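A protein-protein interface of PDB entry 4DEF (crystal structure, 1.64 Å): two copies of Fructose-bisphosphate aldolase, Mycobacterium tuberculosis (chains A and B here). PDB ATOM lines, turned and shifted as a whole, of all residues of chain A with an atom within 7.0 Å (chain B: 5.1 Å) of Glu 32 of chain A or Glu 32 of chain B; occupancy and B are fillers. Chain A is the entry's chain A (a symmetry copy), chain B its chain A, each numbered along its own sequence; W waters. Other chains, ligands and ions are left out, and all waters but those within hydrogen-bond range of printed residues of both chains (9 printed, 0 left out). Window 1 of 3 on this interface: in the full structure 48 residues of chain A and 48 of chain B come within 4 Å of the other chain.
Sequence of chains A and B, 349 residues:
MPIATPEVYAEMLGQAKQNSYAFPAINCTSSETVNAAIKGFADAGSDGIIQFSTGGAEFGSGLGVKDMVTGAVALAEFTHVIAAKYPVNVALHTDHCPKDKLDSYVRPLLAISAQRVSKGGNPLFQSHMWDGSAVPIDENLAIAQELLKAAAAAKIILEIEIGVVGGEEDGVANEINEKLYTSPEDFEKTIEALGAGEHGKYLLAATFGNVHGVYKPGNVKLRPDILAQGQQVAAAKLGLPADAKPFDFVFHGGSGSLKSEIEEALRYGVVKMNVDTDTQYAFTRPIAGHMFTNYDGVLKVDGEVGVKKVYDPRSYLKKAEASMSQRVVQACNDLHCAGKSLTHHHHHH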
ATOM      1  N   CYS A  28      -4.063 -12.366  22.618  1.00  0.00           N
ATOM      2  CA  CYS A  28      -5.499 -12.531  22.814  1.00  0.00           C
ATOM      3  C   CYS A  28      -6.275 -11.698  21.811  1.00  0.00           C
ATOM      4  O   CYS A  28      -5.768 -10.706  21.266  1.00  0.00           O
ATOM      5  CB  CYS A  28      -5.895 -12.135  24.233  1.00  0.00           C
ATOM      6  SG  CYS A  28      -5.123 -13.165  25.498  1.00  0.00           S
ATOM      7  N   THR A  29      -7.526 -12.087  21.579  1.00  0.00           N
ATOM      8  CA  THR A  29      -8.342 -11.476  20.524  1.00  0.00           C
ATOM      9  C   THR A  29      -9.784 -11.241  20.987  1.00  0.00           C
ATOM     10  O   THR A  29     -10.612 -10.781  20.217  1.00  0.00           O
ATOM     11  CB  THR A  29      -8.411 -12.422  19.300  1.00  0.00           C
ATOM     12  OG1 THR A  29      -8.830 -13.731  19.736  1.00  0.00           O
ATOM     13  CG2 THR A  29      -7.044 -12.550  18.624  1.00  0.00           C
ATOM     14  N   SER A  30     -10.098 -11.554  22.244  1.00  0.00           N
ATOM     15  CA  SER A  30     -11.489 -11.627  22.646  1.00  0.00           C
ATOM     16  C   SER A  30     -11.601 -11.712  24.141  1.00  0.00           C
ATOM     17  O   SER A  30     -10.624 -11.985  24.824  1.00  0.00           O
ATOM     18  CB  SER A  30     -12.135 -12.895  22.078  1.00  0.00           C
ATOM     19  OG  SER A  30     -11.485 -14.055  22.561  1.00  0.00           O
ATOM     20  N   SER A  31     -12.822 -11.539  24.621  1.00  0.00           N
ATOM     21  CA  SER A  31     -13.121 -11.733  26.033  1.00  0.00           C
ATOM     22  C   SER A  31     -12.752 -13.149  26.500  1.00  0.00           C
ATOM     23  O   SER A  31     -12.168 -13.329  27.597  1.00  0.00           O
ATOM     24  CB  SER A  31     -14.599 -11.427  26.299  1.00  0.00           C
ATOM     25  OG  SER A  31     -15.491 -12.209  25.492  1.00  0.00           O
ATOM     26  N   GLU A  32     -13.084 -14.155  25.688  1.00  0.00           N
ATOM     27  CA  GLU A  32     -12.749 -15.545  26.050  1.00  0.00           C
ATOM     28  C   GLU A  32     -11.256 -15.804  26.174  1.00  0.00           C
ATOM     29  O   GLU A  32     -10.820 -16.477  27.120  1.00  0.00           O
ATOM     30  CB  GLU A  32     -13.366 -16.554  25.076  1.00  0.00           C
ATOM     31  CG  GLU A  32     -14.885 -16.537  25.079  1.00  0.00           C
ATOM     32  CD  GLU A  32     -15.475 -15.709  23.952  1.00  0.00           C
ATOM     33  OE1 GLU A  32     -14.837 -14.729  23.493  1.00  0.00           O
ATOM     34  OE2 GLU A  32     -16.598 -16.054  23.534  1.00  0.00           O
ATOM     35  N   THR A  33     -10.481 -15.312  25.210  1.00  0.00           N
ATOM     36  CA  THR A  33      -9.035 -15.557  25.206  1.00  0.00           C
ATOM     37  C   THR A  33      -8.345 -14.764  26.335  1.00  0.00           C
ATOM     38  O   THR A  33      -7.456 -15.295  26.998  1.00  0.00           O
ATOM     39  CB  THR A  33      -8.393 -15.340  23.811  1.00  0.00           C
ATOM     40  OG1 THR A  33      -8.759 -14.051  23.307  1.00  0.00           O
ATOM     41  CG2 THR A  33      -8.864 -16.436  22.849  1.00  0.00           C
ATOM     42  N   VAL A  34      -8.780 -13.519  26.579  1.00  0.00           N
ATOM     43  CA  VAL A  34      -8.289 -12.746  27.730  1.00  0.00           C
ATOM     44  C   VAL A  34      -8.582 -13.527  29.014  1.00  0.00           C
ATOM     45  O   VAL A  34      -7.690 -13.734  29.860  1.00  0.00           O
ATOM     46  CB  VAL A  34      -8.912 -11.332  27.799  1.00  0.00           C
ATOM     47  CG1 VAL A  34      -8.651 -10.694  29.163  1.00  0.00           C
ATOM     48  CG2 VAL A  34      -8.339 -10.449  26.691  1.00  0.00           C
ATOM     49  N   ASN A  35      -9.825 -13.968  29.164  1.00  0.00           N
ATOM     50  CA  ASN A  35     -10.186 -14.735  30.372  1.00  0.00           C
ATOM     51  C   ASN A  35      -9.352 -15.997  30.555  1.00  0.00           C
ATOM     52  O   ASN A  35      -8.895 -16.284  31.677  1.00  0.00           O
ATOM     53  CB  ASN A  35     -11.674 -15.064  30.391  1.00  0.00           C
ATOM     54  CG  ASN A  35     -12.520 -13.908  30.900  1.00  0.00           C
ATOM     55  OD1 ASN A  35     -12.044 -13.049  31.644  1.00  0.00           O
ATOM     56  ND2 ASN A  35     -13.773 -13.887  30.511  1.00  0.00           N
ATOM     57  N   ALA A  36      -9.126 -16.730  29.465  1.00  0.00           N
ATOM     58  CA  ALA A  36      -8.282 -17.943  29.499  1.00  0.00           C
ATOM     59  C   ALA A  36      -6.845 -17.631  29.913  1.00  0.00           C
ATOM     60  O   ALA A  36      -6.230 -18.370  30.683  1.00  0.00           O
ATOM     61  CB  ALA A  36      -8.304 -18.649  28.138  1.00  0.00           C
ATOM     62  N   ALA A  37      -6.294 -16.547  29.379  1.00  0.00           N
ATOM     63  CA  ALA A  37      -4.933 -16.181  29.693  1.00  0.00           C
ATOM     64  C   ALA A  37      -4.761 -15.798  31.138  1.00  0.00           C
ATOM     65  O   ALA A  37      -3.812 -16.264  31.769  1.00  0.00           O
ATOM     66  CB  ALA A  37      -4.451 -15.059  28.791  1.00  0.00           C
ATOM     67  N   PHE A  59      -9.769  -7.502  14.738  1.00  0.00           N
ATOM     68  CA  PHE A  59     -10.786  -8.531  15.029  1.00  0.00           C
ATOM     69  C   PHE A  59     -11.619  -8.169  16.268  1.00  0.00           C
ATOM     70  O   PHE A  59     -12.854  -8.291  16.269  1.00  0.00           O
ATOM     71  CB  PHE A  59     -10.118  -9.896  15.213  1.00  0.00           C
ATOM     72  CG  PHE A  59     -11.067 -10.972  15.687  1.00  0.00           C
ATOM     73  CD1 PHE A  59     -11.870 -11.659  14.785  1.00  0.00           C
ATOM     74  CD2 PHE A  59     -11.171 -11.253  17.043  1.00  0.00           C
ATOM     75  CE1 PHE A  59     -12.760 -12.634  15.229  1.00  0.00           C
ATOM     76  CE2 PHE A  59     -12.056 -12.223  17.493  1.00  0.00           C
ATOM     77  CZ  PHE A  59     -12.853 -12.907  16.596  1.00  0.00           C
ATOM     78  N   GLY A  60     -10.940  -7.717  17.317  1.00  0.00           N
ATOM     79  CA  GLY A  60     -11.619  -7.259  18.534  1.00  0.00           C
ATOM     80  C   GLY A  60     -12.627  -6.139  18.341  1.00  0.00           C
ATOM     81  O   GLY A  60     -13.613  -6.041  19.081  1.00  0.00           O
ATOM     82  N   GLY A  62     -14.584  -5.811  15.802  1.00  0.00           N
ATOM     83  CA  GLY A  62     -15.725  -6.327  15.042  1.00  0.00           C
ATOM     84  C   GLY A  62     -15.667  -6.017  13.552  1.00  0.00           C
ATOM     85  O   GLY A  62     -15.013  -5.057  13.127  1.00  0.00           O
ATOM     86  N   LEU A  75     -10.859  -4.061  24.238  1.00  0.00           N
ATOM     87  CA  LEU A  75     -10.335  -5.258  24.918  1.00  0.00           C
ATOM     88  C   LEU A  75      -9.545  -4.882  26.168  1.00  0.00           C
ATOM     89  O   LEU A  75      -9.619  -5.583  27.188  1.00  0.00           O
ATOM     90  CB  LEU A  75      -9.498  -6.127  23.967  1.00  0.00           C
ATOM     91  CG  LEU A  75     -10.266  -6.862  22.863  1.00  0.00           C
ATOM     92  CD1 LEU A  75      -9.280  -7.461  21.876  1.00  0.00           C
ATOM     93  CD2 LEU A  75     -11.192  -7.939  23.423  1.00  0.00           C
ATOM     94  N   PHE A  78     -12.103  -4.095  28.908  1.00  0.00           N
ATOM     95  CA  PHE A  78     -12.597  -5.377  29.407  1.00  0.00           C
ATOM     96  C   PHE A  78     -11.571  -5.993  30.367  1.00  0.00           C
ATOM     97  O   PHE A  78     -11.935  -6.449  31.457  1.00  0.00           O
ATOM     98  CB  PHE A  78     -12.884  -6.333  28.237  1.00  0.00           C
ATOM     99  CG  PHE A  78     -13.239  -7.736  28.669  1.00  0.00           C
ATOM    100  CD1 PHE A  78     -14.566  -8.084  28.897  1.00  0.00           C
ATOM    101  CD2 PHE A  78     -12.249  -8.702  28.809  1.00  0.00           C
ATOM    102  CE1 PHE A  78     -14.896  -9.379  29.292  1.00  0.00           C
ATOM    103  CE2 PHE A  78     -12.573  -9.993  29.211  1.00  0.00           C
ATOM    104  CZ  PHE A  78     -13.898 -10.324  29.453  1.00  0.00           C
ATOM    105  N   PHE A 283      -6.892 -23.523  22.341  1.00  0.00           N
ATOM    106  CA  PHE A 283      -8.240 -22.963  22.399  1.00  0.00           C
ATOM    107  C   PHE A 283      -9.171 -23.700  21.423  1.00  0.00           C
ATOM    108  O   PHE A 283     -10.284 -24.087  21.773  1.00  0.00           O
ATOM    109  CB  PHE A 283      -8.185 -21.471  22.058  1.00  0.00           C
ATOM    110  CG  PHE A 283      -9.479 -20.747  22.279  1.00  0.00           C
ATOM    111  CD1 PHE A 283      -9.770 -20.183  23.529  1.00  0.00           C
ATOM    112  CD2 PHE A 283     -10.404 -20.603  21.243  1.00  0.00           C
ATOM    113  CE1 PHE A 283     -10.965 -19.505  23.738  1.00  0.00           C
ATOM    114  CE2 PHE A 283     -11.595 -19.918  21.448  1.00  0.00           C
ATOM    115  CZ  PHE A 283     -11.869 -19.355  22.693  1.00  0.00           C
ATOM    116  N   PRO A 313     -23.133 -21.254  22.587  1.00  0.00           N
ATOM    117  CA  PRO A 313     -21.686 -21.039  22.476  1.00  0.00           C
ATOM    118  C   PRO A 313     -20.926 -21.255  23.775  1.00  0.00           C
ATOM    119  O   PRO A 313     -19.789 -21.705  23.741  1.00  0.00           O
ATOM    120  CB  PRO A 313     -21.593 -19.587  22.027  1.00  0.00           C
ATOM    121  CG  PRO A 313     -22.801 -19.434  21.171  1.00  0.00           C
ATOM    122  CD  PRO A 313     -23.886 -20.191  21.898  1.00  0.00           C
ATOM    123  N   LEU A 317     -17.217 -22.957  24.328  1.00  0.00           N
ATOM    124  CA  LEU A 317     -16.240 -21.900  24.651  1.00  0.00           C
ATOM    125  C   LEU A 317     -15.665 -22.019  26.069  1.00  0.00           C
ATOM    126  O   LEU A 317     -14.524 -21.671  26.298  1.00  0.00           O
ATOM    127  CB  LEU A 317     -16.798 -20.499  24.369  1.00  0.00           C
ATOM    128  CG  LEU A 317     -16.984 -20.224  22.867  1.00  0.00           C
ATOM    129  CD1 LEU A 317     -17.785 -18.945  22.746  1.00  0.00           C
ATOM    130  CD2 LEU A 317     -15.673 -20.142  22.100  1.00  0.00           C
ATOM    131  N   LYS A 318     -16.437 -22.570  27.007  1.00  0.00           N
ATOM    132  CA  LYS A 318     -15.879 -22.870  28.339  1.00  0.00           C
ATOM    133  C   LYS A 318     -14.794 -23.947  28.260  1.00  0.00           C
ATOM    134  O   LYS A 318     -13.802 -23.888  28.988  1.00  0.00           O
ATOM    135  CB  LYS A 318     -16.971 -23.343  29.293  1.00  0.00           C
ATOM    136  CG  LYS A 318     -17.882 -22.251  29.812  1.00  0.00           C
ATOM    137  CD  LYS A 318     -18.732 -22.793  30.963  1.00  0.00           C
ATOM    138  CE  LYS A 318     -19.878 -23.660  30.471  1.00  0.00           C
ATOM    139  NZ  LYS A 318     -20.677 -24.121  31.647  1.00  0.00           N
ATOM    140  N   ALA A 320     -12.930 -24.499  25.541  1.00  0.00           N
ATOM    141  CA  ALA A 320     -11.823 -23.779  24.888  1.00  0.00           C
ATOM    142  C   ALA A 320     -11.009 -22.950  25.879  1.00  0.00           C
ATOM    143  O   ALA A 320      -9.768 -22.963  25.850  1.00  0.00           O
ATOM    144  CB  ALA A 320     -12.380 -22.882  23.793  1.00  0.00           C
ATOM    145  N   GLU A 321     -11.718 -22.235  26.754  1.00  0.00           N
ATOM    146  CA  GLU A 321     -11.094 -21.393  27.773  1.00  0.00           C
ATOM    147  C   GLU A 321     -10.230 -22.227  28.709  1.00  0.00           C
ATOM    148  O   GLU A 321      -9.084 -21.879  28.984  1.00  0.00           O
ATOM    149  CB  GLU A 321     -12.149 -20.645  28.594  1.00  0.00           C
ATOM    150  CG  GLU A 321     -11.531 -19.540  29.436  1.00  0.00           C
ATOM    151  CD  GLU A 321     -12.458 -18.924  30.468  1.00  0.00           C
ATOM    152  OE1 GLU A 321     -11.994 -18.718  31.617  1.00  0.00           O
ATOM    153  OE2 GLU A 321     -13.615 -18.612  30.130  1.00  0.00           O
ATOM    154  N   MET A 324      -7.086 -23.571  26.843  1.00  0.00           N
ATOM    155  CA  MET A 324      -6.099 -22.507  26.646  1.00  0.00           C
ATOM    156  C   MET A 324      -5.407 -22.151  27.975  1.00  0.00           C
ATOM    157  O   MET A 324      -4.188 -21.946  28.014  1.00  0.00           O
ATOM    158  CB  MET A 324      -6.738 -21.268  26.022  1.00  0.00           C
ATOM    159  CG  MET A 324      -5.746 -20.133  25.828  1.00  0.00           C
ATOM    160  SD  MET A 324      -6.435 -18.854  24.765  1.00  0.00           S
ATOM    161  CE  MET A 324      -5.288 -17.528  25.103  1.00  0.00           C
ATOM    162  N   SER A 325      -6.172 -22.104  29.063  1.00  0.00           N
ATOM    163  CA  SER A 325      -5.575 -21.798  30.361  1.00  0.00           C
ATOM    164  C   SER A 325      -4.525 -22.844  30.744  1.00  0.00           C
ATOM    165  O   SER A 325      -3.474 -22.490  31.282  1.00  0.00           O
ATOM    166  CB  SER A 325      -6.640 -21.718  31.438  1.00  0.00           C
ATOM    167  OG  SER A 325      -7.474 -20.586  31.265  1.00  0.00           O
ATOM    168  N   SER B  30     -20.100 -12.322  25.153  1.00  0.00           N
ATOM    169  CA  SER B  30     -18.704 -12.199  24.779  1.00  0.00           C
ATOM    170  C   SER B  30     -18.506 -11.020  23.871  1.00  0.00           C
ATOM    171  O   SER B  30     -19.461 -10.483  23.329  1.00  0.00           O
ATOM    172  CB  SER B  30     -18.258 -13.441  24.001  1.00  0.00           C
ATOM    173  OG  SER B  30     -19.012 -13.595  22.814  1.00  0.00           O
ATOM    174  N   SER B  31     -17.244 -10.678  23.667  1.00  0.00           N
ATOM    175  CA  SER B  31     -16.879  -9.649  22.703  1.00  0.00           C
ATOM    176  C   SER B  31     -17.387  -9.989  21.294  1.00  0.00           C
ATOM    177  O   SER B  31     -17.916  -9.107  20.573  1.00  0.00           O
ATOM    178  CB  SER B  31     -15.360  -9.443  22.711  1.00  0.00           C
ATOM    179  OG  SER B  31     -14.626 -10.648  22.453  1.00  0.00           O
ATOM    180  N   GLU B  32     -17.235 -11.253  20.889  1.00  0.00           N
ATOM    181  CA  GLU B  32     -17.713 -11.670  19.557  1.00  0.00           C
ATOM    182  C   GLU B  32     -19.215 -11.526  19.373  1.00  0.00           C
ATOM    183  O   GLU B  32     -19.667 -11.056  18.317  1.00  0.00           O
ATOM    184  CB  GLU B  32     -17.289 -13.104  19.221  1.00  0.00           C
ATOM    185  CG  GLU B  32     -15.783 -13.277  19.134  1.00  0.00           C
ATOM    186  CD  GLU B  32     -15.171 -13.832  20.408  1.00  0.00           C
ATOM    187  OE1 GLU B  32     -15.713 -13.600  21.517  1.00  0.00           O
ATOM    188  OE2 GLU B  32     -14.128 -14.505  20.280  1.00  0.00           O
ATOM    189  N   THR B  33     -19.985 -11.962  20.367  1.00  0.00           N
ATOM    190  CA  THR B  33     -21.447 -11.922  20.260  1.00  0.00           C
ATOM    191  C   THR B  33     -21.960 -10.468  20.336  1.00  0.00           C
ATOM    192  O   THR B  33     -22.861 -10.100  19.585  1.00  0.00           O
ATOM    193  CB  THR B  33     -22.149 -12.881  21.257  1.00  0.00           C
ATOM    194  OG1 THR B  33     -21.661 -12.640  22.582  1.00  0.00           O
ATOM    195  CG2 THR B  33     -21.879 -14.335  20.852  1.00  0.00           C
ATOM    196  N   VAL B  34     -21.360  -9.640  21.203  1.00  0.00           N
ATOM    197  CA  VAL B  34     -21.677  -8.203  21.237  1.00  0.00           C
ATOM    198  C   VAL B  34     -21.398  -7.601  19.857  1.00  0.00           C
ATOM    199  O   VAL B  34     -22.251  -6.904  19.275  1.00  0.00           O
ATOM    200  CB  VAL B  34     -20.882  -7.451  22.330  1.00  0.00           C
ATOM    201  CG1 VAL B  34     -20.973  -5.940  22.119  1.00  0.00           C
ATOM    202  CG2 VAL B  34     -21.415  -7.817  23.715  1.00  0.00           C
ATOM    203  N   ASN B  35     -20.211  -7.870  19.327  1.00  0.00           N
ATOM    204  CA  ASN B  35     -19.868  -7.332  17.996  1.00  0.00           C
ATOM    205  C   ASN B  35     -20.836  -7.767  16.903  1.00  0.00           C
ATOM    206  O   ASN B  35     -21.251  -6.937  16.072  1.00  0.00           O
ATOM    207  CB  ASN B  35     -18.434  -7.678  17.615  1.00  0.00           C
ATOM    208  CG  ASN B  35     -17.421  -6.728  18.236  1.00  0.00           C
ATOM    209  OD1 ASN B  35     -17.738  -5.585  18.566  1.00  0.00           O
ATOM    210  ND2 ASN B  35     -16.203  -7.192  18.387  1.00  0.00           N
ATOM    211  N   ALA B  36     -21.222  -9.042  16.916  1.00  0.00           N
ATOM    212  CA  ALA B  36     -22.204  -9.573  15.947  1.00  0.00           C
ATOM    213  C   ALA B  36     -23.562  -8.883  16.070  1.00  0.00           C
ATOM    214  O   ALA B  36     -24.210  -8.573  15.070  1.00  0.00           O
ATOM    215  CB  ALA B  36     -22.358 -11.089  16.116  1.00  0.00           C
ATOM    216  N   ALA B  37     -24.009  -8.668  17.302  1.00  0.00           N
ATOM    217  CA  ALA B  37     -25.291  -8.040  17.520  1.00  0.00           C
ATOM    218  C   ALA B  37     -25.320  -6.612  17.046  1.00  0.00           C
ATOM    219  O   ALA B  37     -26.276  -6.228  16.371  1.00  0.00           O
ATOM    220  CB  ALA B  37     -25.691  -8.117  18.983  1.00  0.00           C
ATOM    221  N   PHE B  59     -20.422 -16.292  32.704  1.00  0.00           N
ATOM    222  CA  PHE B  59     -19.522 -16.738  31.623  1.00  0.00           C
ATOM    223  C   PHE B  59     -18.572 -15.616  31.179  1.00  0.00           C
ATOM    224  O   PHE B  59     -17.363 -15.832  30.997  1.00  0.00           O
ATOM    225  CB  PHE B  59     -20.338 -17.249  30.432  1.00  0.00           C
ATOM    226  CG  PHE B  59     -19.499 -17.559  29.215  1.00  0.00           C
ATOM    227  CD1 PHE B  59     -18.847 -18.779  29.094  1.00  0.00           C
ATOM    228  CD2 PHE B  59     -19.342 -16.601  28.222  1.00  0.00           C
ATOM    229  CE1 PHE B  59     -18.056 -19.053  27.981  1.00  0.00           C
ATOM    230  CE2 PHE B  59     -18.555 -16.865  27.110  1.00  0.00           C
ATOM    231  CZ  PHE B  59     -17.907 -18.080  26.989  1.00  0.00           C
ATOM    232  N   PHE B 283     -24.733 -18.382  15.388  1.00  0.00           N
ATOM    233  CA  PHE B 283     -23.326 -18.194  15.732  1.00  0.00           C
ATOM    234  C   PHE B 283     -22.558 -19.518  15.602  1.00  0.00           C
ATOM    235  O   PHE B 283     -21.481 -19.576  15.014  1.00  0.00           O
ATOM    236  CB  PHE B 283     -23.220 -17.655  17.162  1.00  0.00           C
ATOM    237  CG  PHE B 283     -21.836 -17.235  17.555  1.00  0.00           C
ATOM    238  CD1 PHE B 283     -21.397 -15.927  17.309  1.00  0.00           C
ATOM    239  CD2 PHE B 283     -20.970 -18.129  18.188  1.00  0.00           C
ATOM    240  CE1 PHE B 283     -20.117 -15.529  17.676  1.00  0.00           C
ATOM    241  CE2 PHE B 283     -19.693 -17.730  18.565  1.00  0.00           C
ATOM    242  CZ  PHE B 283     -19.272 -16.425  18.322  1.00  0.00           C
ATOM    243  N   LEU B 317     -14.308 -17.690  14.076  1.00  0.00           N
ATOM    244  CA  LEU B 317     -15.126 -16.725  14.838  1.00  0.00           C
ATOM    245  C   LEU B 317     -15.616 -15.545  13.989  1.00  0.00           C
ATOM    246  O   LEU B 317     -16.689 -15.025  14.225  1.00  0.00           O
ATOM    247  CB  LEU B 317     -14.420 -16.263  16.118  1.00  0.00           C
ATOM    248  CG  LEU B 317     -14.301 -17.381  17.168  1.00  0.00           C
ATOM    249  CD1 LEU B 317     -13.359 -16.881  18.244  1.00  0.00           C
ATOM    250  CD2 LEU B 317     -15.639 -17.811  17.749  1.00  0.00           C
ATOM    251  N   GLU B 321     -19.506 -14.611  13.689  1.00  0.00           N
ATOM    252  CA  GLU B 321     -19.955 -13.230  13.861  1.00  0.00           C
ATOM    253  C   GLU B 321     -20.850 -12.804  12.707  1.00  0.00           C
ATOM    254  O   GLU B 321     -21.925 -12.246  12.918  1.00  0.00           O
ATOM    255  CB  GLU B 321     -18.765 -12.271  13.957  1.00  0.00           C
ATOM    256  CG  GLU B 321     -19.186 -10.895  14.445  1.00  0.00           C
ATOM    257  CD  GLU B 321     -18.125  -9.816  14.322  1.00  0.00           C
ATOM    258  OE1 GLU B 321     -18.484  -8.695  13.885  1.00  0.00           O
ATOM    259  OE2 GLU B 321     -16.963 -10.068  14.692  1.00  0.00           O
HETATM  260  O   HOH W   1     -18.325 -15.707  21.564  1.00  0.00           O
HETATM  261  O   HOH W   2     -14.720  -9.738  17.809  1.00  0.00           O
HETATM  262  O   HOH W   3     -15.591 -15.573  28.819  1.00  0.00           O
HETATM  263  O   HOH W   4     -12.505 -16.160  21.549  1.00  0.00           O
HETATM  264  O   HOH W   5     -16.228 -18.419  31.281  1.00  0.00           O
HETATM  265  O   HOH W   6     -10.924 -15.219  19.410  1.00  0.00           O
HETATM  266  O   HOH W   7     -14.276  -9.329  14.041  1.00  0.00           O
HETATM  267  O   HOH W   8     -19.916 -16.773  23.635  1.00  0.00           O
HETATM  268  O   HOH W   9     -13.485 -10.417  20.149  1.00  0.00           O
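Water W9 bridges OG of Ser 31 of chain B (2.6 Å) and O of Thr 29 of chain A (2.9 Å). Water W6 lies within hydrogen-bond range of the side-chain hydroxyl of Thr 29 of chain A, the side-chain carboxylate of Glu 32 of chain B and the side-chain hydroxyl of Ser 30 of chain A. Water W3 bridges O of Phe 59 of chain B and ND2 of Asn 35 of chain A. Water W7 lies within hydrogen-bond range of the backbone carbonyl oxygen (O) of Phe 59 of chain A (2.8 Å) and the side-chain carboxylate (OE2) of Glu 321 of chain B (2.9 Å). Water W5 bridges the backbone carbonyl oxygen of Phe 59 of chain B (2.8 Å) and the side-chain carboxylate of Glu 321 of chain A (2.9 Å). Water W8 bridges OE2 of Glu 32 of chain A (3.4 Å) and OG of Ser 30 of chain B (3.4 Å).
Ser 30 of chain A touches Ser 31 of chain B, and with the chains exchanged Ser 31 of chain A touches Ser 30 of chain B. Glu 32 of chain B touches its own counterpart, Glu 32 of chain A. Glu 32 of chain A touches Phe 59 of chain B, and with the chains exchanged Phe 59 of chain A touches Glu 32 of chain B. Phe 59 of chain A touches Leu 317 of chain B, and with the chains exchanged Leu 317 of chain A touches Phe 59 of chain B. 12 positions are printed for both chains. Of the 15 pairs that touch across the chains among the printed residues, 10 have their exchanged pair printed and touching as well.
CA of Ser 30 of chain A touches OG of Ser 31 of chain B, 3.3 Å away. Ser 30 of chain A touches Glu 32 of chain B. Ser 31 of chain A touches Ser 30 of chain B (OG to CA, 3.3 Å). CZ of Phe 59 of chain B touches CG of Glu 32 of chain A, at 3.9 Å. Glu 32 of chain B touches Phe 59 of chain A. Phe 59 of chain A touches Leu 317 of chain B (CZ to CB, 3.7 Å). Glu 321 of chain B touches Gly 62 of chain A. Pro 313 of chain A touches Phe 283 of chain B (CG to CD2, 3.7 Å). Phe 59 of chain B touches Leu 317 of chain A (CZ to CB, 3.7 Å). CG of Lys 318 of chain A touches CD1 of Phe 59 of chain B, 3.7 Å away.
The side-chain hydroxyl (OG) of Ser 30 of chain B lies within hydrogen-bond range of the side-chain hydroxyl (OG1) of Thr 33 of chain B, 2.8 Å away. ND2 of Asn 35 of chain A sits close to O of Ser 31 of chain A (3.4 Å). OG1 of Thr 33 of chain A is in hydrogen-bond range of OG of Ser 30 of chain A. The side-chain hydroxyl (OG) of Ser 31 of chain B lies within hydrogen-bond range of the side-chain carboxylate (OE1) of Glu 32 of chain B (3.3 Å). ND2 of Asn 35 of chain B sits close to O of Ser 31 of chain B, at 3.4 Å. The side-chain carboxylate of Glu 32 of chain A is in hydrogen-bond range of the side-chain hydroxyl of Ser 31 of chain A.
Of the 12 printed residues of chain B, 8 touch a printed residue of chain A. Hydrophobic or aromatic side chains of chain B within 4 Å of the printed part of chain A: Phe 59, Phe 283 and Leu 317. Of the 23 printed residues of chain A, 9 touch a printed residue of chain B. Hydrophobic or aromatic side chains of chain A within 4 Å of the printed part of chain B: Phe 59, Pro 313 and Leu 317. Among the printed residues, 15 pairs touch across the chains.
OE1 of Glu 32 of chain B lies close to OE1 of Glu 32 of chain A (2.4 Å). The side-chain amide nitrogen (ND2) of Asn 35 of chain B lies close to the backbone NH (N) of Gly 62 of chain A, at 3.3 Å. N of Ser 31 of chain B lies within hydrogen-bond range of OG of Ser 31 of chain A, 3.0 Å away. The side-chain amide nitrogen (ND2) of Asn 35 of chain B sits at hydrogen-bond distance from the backbone carbonyl oxygen (O) of Gly 60 of chain A, at 2.9 Å.
Of chain B, only Ser 30 (3.1 Å), Glu 32 (2.4 Å) and Phe 59 (3.9 Å) come within 4 Å of Glu 32 of chain A. Of the printed residues of chain B, Ser 30 of chain A touches Ser 31 (3.3 Å) and Glu 32 (3.1 Å). Of the printed residues of chain B, Phe 59 of chain A touches Glu 32 (3.9 Å) and Leu 317 (3.7 Å). Of the printed residues of chain A, Leu 317 of chain B touches Phe 59. The nearest residue of chain B that does not touch Glu 32 of chain A is Ser 31 of chain B (4.2 Å). The nearest printed residue of chain B that does not touch Phe 59 of chain A is Asn 35 of chain B (4.1 Å).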
